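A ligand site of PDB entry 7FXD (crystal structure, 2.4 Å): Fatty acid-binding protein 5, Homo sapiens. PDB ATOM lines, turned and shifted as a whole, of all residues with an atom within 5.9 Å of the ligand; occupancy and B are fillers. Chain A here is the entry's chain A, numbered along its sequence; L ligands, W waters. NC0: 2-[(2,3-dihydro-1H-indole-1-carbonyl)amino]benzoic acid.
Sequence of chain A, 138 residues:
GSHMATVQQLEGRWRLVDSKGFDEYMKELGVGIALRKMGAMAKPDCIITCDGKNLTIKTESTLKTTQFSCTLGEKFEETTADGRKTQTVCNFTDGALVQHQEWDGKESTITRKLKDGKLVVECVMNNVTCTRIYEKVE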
ATOM      1  N   LEU A  16     -30.395 -25.442  25.150  1.00  0.00           N
ATOM      2  CA  LEU A  16     -30.694 -24.570  23.989  1.00  0.00           C
ATOM      3  C   LEU A  16     -30.701 -25.340  22.659  1.00  0.00           C
ATOM      4  O   LEU A  16     -29.786 -26.122  22.431  1.00  0.00           O
ATOM      5  CB  LEU A  16     -29.700 -23.404  23.920  1.00  0.00           C
ATOM      6  CG  LEU A  16     -29.924 -22.358  22.819  1.00  0.00           C
ATOM      7  CD1 LEU A  16     -30.947 -21.327  23.232  1.00  0.00           C
ATOM      8  CD2 LEU A  16     -28.612 -21.703  22.421  1.00  0.00           C
ATOM      9  N   PHE A  22     -30.321 -13.073  19.224  1.00  0.00           N
ATOM     10  CA  PHE A  22     -29.480 -12.997  20.419  1.00  0.00           C
ATOM     11  C   PHE A  22     -28.420 -11.893  20.284  1.00  0.00           C
ATOM     12  O   PHE A  22     -28.307 -11.063  21.202  1.00  0.00           O
ATOM     13  CB  PHE A  22     -28.912 -14.387  20.836  1.00  0.00           C
ATOM     14  CG  PHE A  22     -28.338 -14.484  22.229  1.00  0.00           C
ATOM     15  CD1 PHE A  22     -29.102 -14.138  23.347  1.00  0.00           C
ATOM     16  CD2 PHE A  22     -27.030 -14.918  22.435  1.00  0.00           C
ATOM     17  CE1 PHE A  22     -28.573 -14.231  24.637  1.00  0.00           C
ATOM     18  CE2 PHE A  22     -26.500 -14.999  23.732  1.00  0.00           C
ATOM     19  CZ  PHE A  22     -27.278 -14.670  24.824  1.00  0.00           C
ATOM     20  N   TYR A  25     -29.987  -8.374  20.562  1.00  0.00           N
ATOM     21  CA  TYR A  25     -30.356  -8.179  21.962  1.00  0.00           C
ATOM     22  C   TYR A  25     -29.123  -7.833  22.842  1.00  0.00           C
ATOM     23  O   TYR A  25     -29.179  -6.918  23.656  1.00  0.00           O
ATOM     24  CB  TYR A  25     -31.164  -9.389  22.480  1.00  0.00           C
ATOM     25  CG  TYR A  25     -31.493  -9.332  23.949  1.00  0.00           C
ATOM     26  CD1 TYR A  25     -32.465  -8.446  24.431  1.00  0.00           C
ATOM     27  CD2 TYR A  25     -30.778 -10.071  24.880  1.00  0.00           C
ATOM     28  CE1 TYR A  25     -32.725  -8.328  25.790  1.00  0.00           C
ATOM     29  CE2 TYR A  25     -31.065  -9.994  26.244  1.00  0.00           C
ATOM     30  CZ  TYR A  25     -32.039  -9.123  26.692  1.00  0.00           C
ATOM     31  OH  TYR A  25     -32.312  -9.022  28.025  1.00  0.00           O
ATOM     32  N   MET A  38     -18.631 -14.828  21.508  1.00  0.00           N
ATOM     33  CA  MET A  38     -18.527 -15.893  22.493  1.00  0.00           C
ATOM     34  C   MET A  38     -19.917 -16.369  22.864  1.00  0.00           C
ATOM     35  O   MET A  38     -20.197 -17.558  22.738  1.00  0.00           O
ATOM     36  CB  MET A  38     -17.838 -15.384  23.772  1.00  0.00           C
ATOM     37  CG  MET A  38     -16.504 -14.758  23.545  1.00  0.00           C
ATOM     38  SD  MET A  38     -15.166 -15.960  23.421  1.00  0.00           S
ATOM     39  CE  MET A  38     -14.691 -16.092  25.188  1.00  0.00           C
ATOM     40  N   GLY A  39     -20.792 -15.439  23.336  1.00  0.00           N
ATOM     41  CA  GLY A  39     -22.173 -15.686  23.756  1.00  0.00           C
ATOM     42  C   GLY A  39     -22.988 -16.401  22.685  1.00  0.00           C
ATOM     43  O   GLY A  39     -23.779 -17.287  22.996  1.00  0.00           O
ATOM     44  N   ALA A  40     -22.776 -16.033  21.413  1.00  0.00           N
ATOM     45  CA  ALA A  40     -23.443 -16.647  20.280  1.00  0.00           C
ATOM     46  C   ALA A  40     -22.935 -18.086  20.065  1.00  0.00           C
ATOM     47  O   ALA A  40     -23.707 -18.932  19.625  1.00  0.00           O
ATOM     48  CB  ALA A  40     -23.222 -15.815  19.026  1.00  0.00           C
ATOM     49  N   ALA A  42     -21.794 -20.225  22.537  1.00  0.00           N
ATOM     50  CA  ALA A  42     -22.290 -21.039  23.650  1.00  0.00           C
ATOM     51  C   ALA A  42     -23.638 -21.666  23.388  1.00  0.00           C
ATOM     52  O   ALA A  42     -24.471 -21.130  22.629  1.00  0.00           O
ATOM     53  CB  ALA A  42     -22.336 -20.217  24.923  1.00  0.00           C
ATOM     54  N   LYS A  43     -23.813 -22.855  23.928  1.00  0.00           N
ATOM     55  CA  LYS A  43     -25.057 -23.616  23.822  1.00  0.00           C
ATOM     56  C   LYS A  43     -25.402 -23.969  25.290  1.00  0.00           C
ATOM     57  O   LYS A  43     -25.130 -25.077  25.736  1.00  0.00           O
ATOM     58  CB  LYS A  43     -24.847 -24.858  22.931  1.00  0.00           C
ATOM     59  CG  LYS A  43     -26.162 -25.552  22.499  1.00  0.00           C
ATOM     60  CD  LYS A  43     -26.294 -26.952  23.113  1.00  0.00           C
ATOM     61  CE  LYS A  43     -25.856 -28.092  22.217  1.00  0.00           C
ATOM     62  NZ  LYS A  43     -26.913 -28.446  21.222  1.00  0.00           N
ATOM     63  N   PRO A  44     -25.891 -22.989  26.080  1.00  0.00           N
ATOM     64  CA  PRO A  44     -26.114 -23.283  27.505  1.00  0.00           C
ATOM     65  C   PRO A  44     -27.283 -24.197  27.929  1.00  0.00           C
ATOM     66  O   PRO A  44     -28.268 -24.397  27.209  1.00  0.00           O
ATOM     67  CB  PRO A  44     -26.211 -21.892  28.156  1.00  0.00           C
ATOM     68  CG  PRO A  44     -26.368 -20.908  27.004  1.00  0.00           C
ATOM     69  CD  PRO A  44     -26.435 -21.669  25.722  1.00  0.00           C
ATOM     70  N   THR A  59     -27.845 -20.597  34.580  1.00  0.00           N
ATOM     71  CA  THR A  59     -27.441 -20.778  33.184  1.00  0.00           C
ATOM     72  C   THR A  59     -26.006 -21.336  33.145  1.00  0.00           C
ATOM     73  O   THR A  59     -25.072 -20.639  33.531  1.00  0.00           O
ATOM     74  CB  THR A  59     -27.676 -19.544  32.292  1.00  0.00           C
ATOM     75  OG1 THR A  59     -29.039 -19.111  32.376  1.00  0.00           O
ATOM     76  CG2 THR A  59     -27.297 -19.811  30.847  1.00  0.00           C
ATOM     77  N   GLU A  60     -25.873 -22.587  32.752  1.00  0.00           N
ATOM     78  CA  GLU A  60     -24.593 -23.277  32.678  1.00  0.00           C
ATOM     79  C   GLU A  60     -24.023 -23.256  31.269  1.00  0.00           C
ATOM     80  O   GLU A  60     -24.666 -23.743  30.325  1.00  0.00           O
ATOM     81  CB  GLU A  60     -24.758 -24.751  33.094  1.00  0.00           C
ATOM     82  CG  GLU A  60     -24.602 -25.011  34.569  1.00  0.00           C
ATOM     83  CD  GLU A  60     -24.516 -26.475  34.941  1.00  0.00           C
ATOM     84  OE1 GLU A  60     -24.598 -27.336  34.036  1.00  0.00           O
ATOM     85  OE2 GLU A  60     -24.399 -26.777  36.152  1.00  0.00           O
ATOM     86  N   SER A  61     -22.818 -22.741  31.124  1.00  0.00           N
ATOM     87  CA  SER A  61     -22.064 -22.773  29.866  1.00  0.00           C
ATOM     88  C   SER A  61     -20.615 -23.016  30.225  1.00  0.00           C
ATOM     89  O   SER A  61     -20.190 -22.585  31.320  1.00  0.00           O
ATOM     90  CB  SER A  61     -22.173 -21.460  29.115  1.00  0.00           C
ATOM     91  OG  SER A  61     -21.407 -21.554  27.916  1.00  0.00           O
ATOM     92  N   LEU A  63     -18.260 -21.466  28.967  1.00  0.00           N
ATOM     93  CA  LEU A  63     -17.749 -20.097  28.948  1.00  0.00           C
ATOM     94  C   LEU A  63     -17.996 -19.324  30.229  1.00  0.00           C
ATOM     95  O   LEU A  63     -17.103 -18.604  30.681  1.00  0.00           O
ATOM     96  CB  LEU A  63     -18.338 -19.304  27.760  1.00  0.00           C
ATOM     97  CG  LEU A  63     -18.083 -19.916  26.363  1.00  0.00           C
ATOM     98  CD1 LEU A  63     -18.928 -19.226  25.324  1.00  0.00           C
ATOM     99  CD2 LEU A  63     -16.605 -19.835  25.987  1.00  0.00           C
ATOM    100  N   LYS A  64     -19.222 -19.394  30.766  1.00  0.00           N
ATOM    101  CA  LYS A  64     -19.672 -18.679  31.961  1.00  0.00           C
ATOM    102  C   LYS A  64     -20.919 -19.322  32.509  1.00  0.00           C
ATOM    103  O   LYS A  64     -21.770 -19.805  31.768  1.00  0.00           O
ATOM    104  CB  LYS A  64     -19.959 -17.188  31.619  1.00  0.00           C
ATOM    105  CG  LYS A  64     -20.309 -16.308  32.830  1.00  0.00           C
ATOM    106  CD  LYS A  64     -19.468 -15.053  32.954  1.00  0.00           C
ATOM    107  CE  LYS A  64     -19.969 -14.247  34.126  1.00  0.00           C
ATOM    108  NZ  LYS A  64     -19.471 -12.846  34.106  1.00  0.00           N
ATOM    109  N   THR A  65     -20.987 -19.371  33.820  1.00  0.00           N
ATOM    110  CA  THR A  65     -22.110 -19.866  34.575  1.00  0.00           C
ATOM    111  C   THR A  65     -22.625 -18.697  35.398  1.00  0.00           C
ATOM    112  O   THR A  65     -21.864 -18.040  36.107  1.00  0.00           O
ATOM    113  CB  THR A  65     -21.737 -21.129  35.378  1.00  0.00           C
ATOM    114  OG1 THR A  65     -21.692 -22.208  34.448  1.00  0.00           O
ATOM    115  CG2 THR A  65     -22.748 -21.451  36.483  1.00  0.00           C
ATOM    116  N   THR A  66     -23.909 -18.451  35.266  1.00  0.00           N
ATOM    117  CA  THR A  66     -24.654 -17.414  35.932  1.00  0.00           C
ATOM    118  C   THR A  66     -25.773 -18.074  36.748  1.00  0.00           C
ATOM    119  O   THR A  66     -26.125 -19.221  36.475  1.00  0.00           O
ATOM    120  CB  THR A  66     -25.061 -16.378  34.855  1.00  0.00           C
ATOM    121  OG1 THR A  66     -24.076 -15.357  34.825  1.00  0.00           O
ATOM    122  CG2 THR A  66     -26.408 -15.761  35.060  1.00  0.00           C
ATOM    123  N   ALA A  81     -24.712 -12.137  33.199  1.00  0.00           N
ATOM    124  CA  ALA A  81     -23.636 -12.766  32.421  1.00  0.00           C
ATOM    125  C   ALA A  81     -22.654 -11.725  31.842  1.00  0.00           C
ATOM    126  O   ALA A  81     -21.443 -11.922  31.892  1.00  0.00           O
ATOM    127  CB  ALA A  81     -24.246 -13.563  31.274  1.00  0.00           C
ATOM    128  N   GLN A  99     -39.501 -11.713  34.122  1.00  0.00           N
ATOM    129  CA  GLN A  99     -38.338 -11.177  34.811  1.00  0.00           C
ATOM    130  C   GLN A  99     -38.030  -9.820  34.199  1.00  0.00           C
ATOM    131  O   GLN A  99     -37.727  -9.717  33.014  1.00  0.00           O
ATOM    132  CB  GLN A  99     -37.157 -12.155  34.701  1.00  0.00           C
ATOM    133  CG  GLN A  99     -35.845 -11.614  35.235  1.00  0.00           C
ATOM    134  CD  GLN A  99     -34.666 -12.435  34.823  1.00  0.00           C
ATOM    135  OE1 GLN A  99     -34.782 -13.380  34.026  1.00  0.00           O
ATOM    136  NE2 GLN A  99     -33.488 -12.083  35.359  1.00  0.00           N
ATOM    137  N   ILE A 110     -37.520 -10.406  30.338  1.00  0.00           N
ATOM    138  CA  ILE A 110     -37.308 -11.794  29.933  1.00  0.00           C
ATOM    139  C   ILE A 110     -38.561 -12.579  30.369  1.00  0.00           C
ATOM    140  O   ILE A 110     -38.895 -12.626  31.554  1.00  0.00           O
ATOM    141  CB  ILE A 110     -35.990 -12.405  30.512  1.00  0.00           C
ATOM    142  CG1 ILE A 110     -34.752 -11.567  30.130  1.00  0.00           C
ATOM    143  CG2 ILE A 110     -35.811 -13.867  30.114  1.00  0.00           C
ATOM    144  CD1 ILE A 110     -34.072 -11.002  31.329  1.00  0.00           C
ATOM    145  N   ARG A 112     -40.506 -16.287  30.109  1.00  0.00           N
ATOM    146  CA  ARG A 112     -40.315 -17.724  29.979  1.00  0.00           C
ATOM    147  C   ARG A 112     -41.655 -18.417  30.119  1.00  0.00           C
ATOM    148  O   ARG A 112     -42.333 -18.280  31.151  1.00  0.00           O
ATOM    149  CB  ARG A 112     -39.328 -18.214  31.056  1.00  0.00           C
ATOM    150  CG  ARG A 112     -37.906 -17.690  30.870  1.00  0.00           C
ATOM    151  CD  ARG A 112     -37.010 -18.140  31.981  1.00  0.00           C
ATOM    152  NE  ARG A 112     -35.664 -17.582  31.857  1.00  0.00           N
ATOM    153  CZ  ARG A 112     -35.251 -16.469  32.467  1.00  0.00           C
ATOM    154  NH1 ARG A 112     -36.095 -15.768  33.206  1.00  0.00           N
ATOM    155  NH2 ARG A 112     -34.016 -16.036  32.296  1.00  0.00           N
ATOM    156  N   VAL A 121     -37.981 -18.606  25.588  1.00  0.00           N
ATOM    157  CA  VAL A 121     -37.429 -17.442  26.282  1.00  0.00           C
ATOM    158  C   VAL A 121     -37.389 -16.238  25.333  1.00  0.00           C
ATOM    159  O   VAL A 121     -36.586 -16.191  24.407  1.00  0.00           O
ATOM    160  CB  VAL A 121     -36.025 -17.757  26.885  1.00  0.00           C
ATOM    161  CG1 VAL A 121     -35.614 -16.713  27.906  1.00  0.00           C
ATOM    162  CG2 VAL A 121     -35.990 -19.159  27.499  1.00  0.00           C
ATOM    163  N   CYS A 123     -36.672 -12.367  25.071  1.00  0.00           N
ATOM    164  CA  CYS A 123     -35.902 -11.293  25.703  1.00  0.00           C
ATOM    165  C   CYS A 123     -36.158 -10.008  24.917  1.00  0.00           C
ATOM    166  O   CYS A 123     -35.995  -9.987  23.692  1.00  0.00           O
ATOM    167  CB  CYS A 123     -34.419 -11.631  25.759  1.00  0.00           C
ATOM    168  SG  CYS A 123     -34.056 -13.273  26.453  1.00  0.00           S
ATOM    169  N   ARG A 132     -35.173 -17.425  22.437  1.00  0.00           N
ATOM    170  CA  ARG A 132     -34.331 -18.599  22.745  1.00  0.00           C
ATOM    171  C   ARG A 132     -35.242 -19.786  23.093  1.00  0.00           C
ATOM    172  O   ARG A 132     -36.101 -19.670  23.978  1.00  0.00           O
ATOM    173  CB  ARG A 132     -33.376 -18.335  23.926  1.00  0.00           C
ATOM    174  CG  ARG A 132     -32.572 -17.057  23.844  1.00  0.00           C
ATOM    175  CD  ARG A 132     -31.268 -17.267  23.104  1.00  0.00           C
ATOM    176  NE  ARG A 132     -30.232 -17.712  24.025  1.00  0.00           N
ATOM    177  CZ  ARG A 132     -29.000 -18.030  23.682  1.00  0.00           C
ATOM    178  NH1 ARG A 132     -28.610 -17.946  22.420  1.00  0.00           N
ATOM    179  NH2 ARG A 132     -28.140 -18.420  24.607  1.00  0.00           N
ATOM    180  N   TYR A 134     -35.508 -23.684  24.371  1.00  0.00           N
ATOM    181  CA  TYR A 134     -34.860 -24.758  25.138  1.00  0.00           C
ATOM    182  C   TYR A 134     -35.675 -26.069  25.094  1.00  0.00           C
ATOM    183  O   TYR A 134     -36.910 -26.062  25.030  1.00  0.00           O
ATOM    184  CB  TYR A 134     -34.594 -24.323  26.595  1.00  0.00           C
ATOM    185  CG  TYR A 134     -33.500 -23.266  26.758  1.00  0.00           C
ATOM    186  CD1 TYR A 134     -33.784 -21.911  26.596  1.00  0.00           C
ATOM    187  CD2 TYR A 134     -32.208 -23.632  27.132  1.00  0.00           C
ATOM    188  CE1 TYR A 134     -32.793 -20.944  26.739  1.00  0.00           C
ATOM    189  CE2 TYR A 134     -31.220 -22.672  27.304  1.00  0.00           C
ATOM    190  CZ  TYR A 134     -31.509 -21.333  27.079  1.00  0.00           C
ATOM    191  OH  TYR A 134     -30.529 -20.371  27.231  1.00  0.00           O
HETATM  192  C1  NC0 L   1     -25.354 -16.894  28.833  1.00  0.00           C
HETATM  193  C12 NC0 L   1     -23.783 -17.748  26.696  1.00  0.00           C
HETATM  194  C13 NC0 L   1     -29.355 -15.347  29.137  1.00  0.00           C
HETATM  195  C14 NC0 L   1     -30.332 -16.043  28.335  1.00  0.00           C
HETATM  196  C15 NC0 L   1     -29.798 -14.190  29.855  1.00  0.00           C
HETATM  197  C16 NC0 L   1     -31.662 -15.589  28.279  1.00  0.00           C
HETATM  198  C17 NC0 L   1     -30.005 -17.188  27.485  1.00  0.00           C
HETATM  199  C18 NC0 L   1     -31.121 -13.776  29.801  1.00  0.00           C
HETATM  200  C19 NC0 L   1     -32.067 -14.466  29.017  1.00  0.00           C
HETATM  201  C3  NC0 L   1     -24.103 -17.597  29.090  1.00  0.00           C
HETATM  202  C4  NC0 L   1     -25.753 -16.613  27.512  1.00  0.00           C
HETATM  203  C5  NC0 L   1     -27.224 -16.011  30.297  1.00  0.00           C
HETATM  204  C6  NC0 L   1     -25.031 -17.033  31.111  1.00  0.00           C
HETATM  205  C7  NC0 L   1     -23.955 -17.687  30.526  1.00  0.00           C
HETATM  206  C8  NC0 L   1     -23.322 -18.011  27.996  1.00  0.00           C
HETATM  207  C9  NC0 L   1     -24.992 -17.096  26.446  1.00  0.00           C
HETATM  208  N10 NC0 L   1     -28.013 -15.729  29.159  1.00  0.00           N
HETATM  209  N2  NC0 L   1     -25.930 -16.592  30.101  1.00  0.00           N
HETATM  210  O11 NC0 L   1     -27.597 -15.781  31.466  1.00  0.00           O
HETATM  211  O20 NC0 L   1     -31.081 -17.809  26.964  1.00  0.00           O
HETATM  212  O21 NC0 L   1     -28.914 -17.656  27.129  1.00  0.00           O
HETATM  213  O   HOH W   1     -27.243 -13.324  32.742  1.00  0.00           O
HETATM  214  O   HOH W   2     -29.984 -11.675  32.063  1.00  0.00           O
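The side-chain hydroxyl of Tyr 134 sits at hydrogen-bond distance from an oxygen (O20) of the ligand (2.6 Å).
NH2 of Arg 132 is in salt-bridge range of O21 of the ligand, 2.7 Å away.
The side-chain hydroxyl (OG) of Ser 61 sits close to the backbone NH (N) of Leu 63, at 3.3 Å.
The side-chain hydroxyl (OG1) of Thr 65 sits at hydrogen-bond distance from the backbone carbonyl oxygen (O) of Ser 61 (3.5 Å).
The backbone NH of Val 121 lies within hydrogen-bond range of the backbone carbonyl oxygen of Arg 132.
O of Thr 66 lies within hydrogen-bond range of N of Thr 59, at 2.9 Å.
O of Gln 99 is in hydrogen-bond range of N of Ile 110, at 2.8 Å.
NZ of Lys 64 lies within hydrogen-bond range of O of Ala 81 (3.1 Å).
Merely in contact with the ligand: Lys 64 (3.3 Å), Ala 42 (3.4 Å), Cys 123 (3.5 Å), Ala 81 (3.6 Å), Thr 59 (3.6 Å), Phe 22 (3.7 Å), Gly 39 (3.7 Å), Thr 66 (3.8 Å), Ser 61 (3.8 Å) and Ile 110 (3.9 Å).
Hydrophobic or aromatic side chains that line the ligand: Phe 22, Ala 42, Ala 81, Ile 110 and Tyr 134.
Within 4 Å of the ligand: Phe 22, Gly 39, Ala 42, Thr 59, Ser 61, Lys 64, Thr 66, Ala 81, Ile 110, Cys 123, Arg 132 and Tyr 134.
Water W1 lies within hydrogen-bond range of an oxygen (O11) of the ligand (2.8 Å) and the backbone NH (N) of Ala 81 (2.8 Å).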
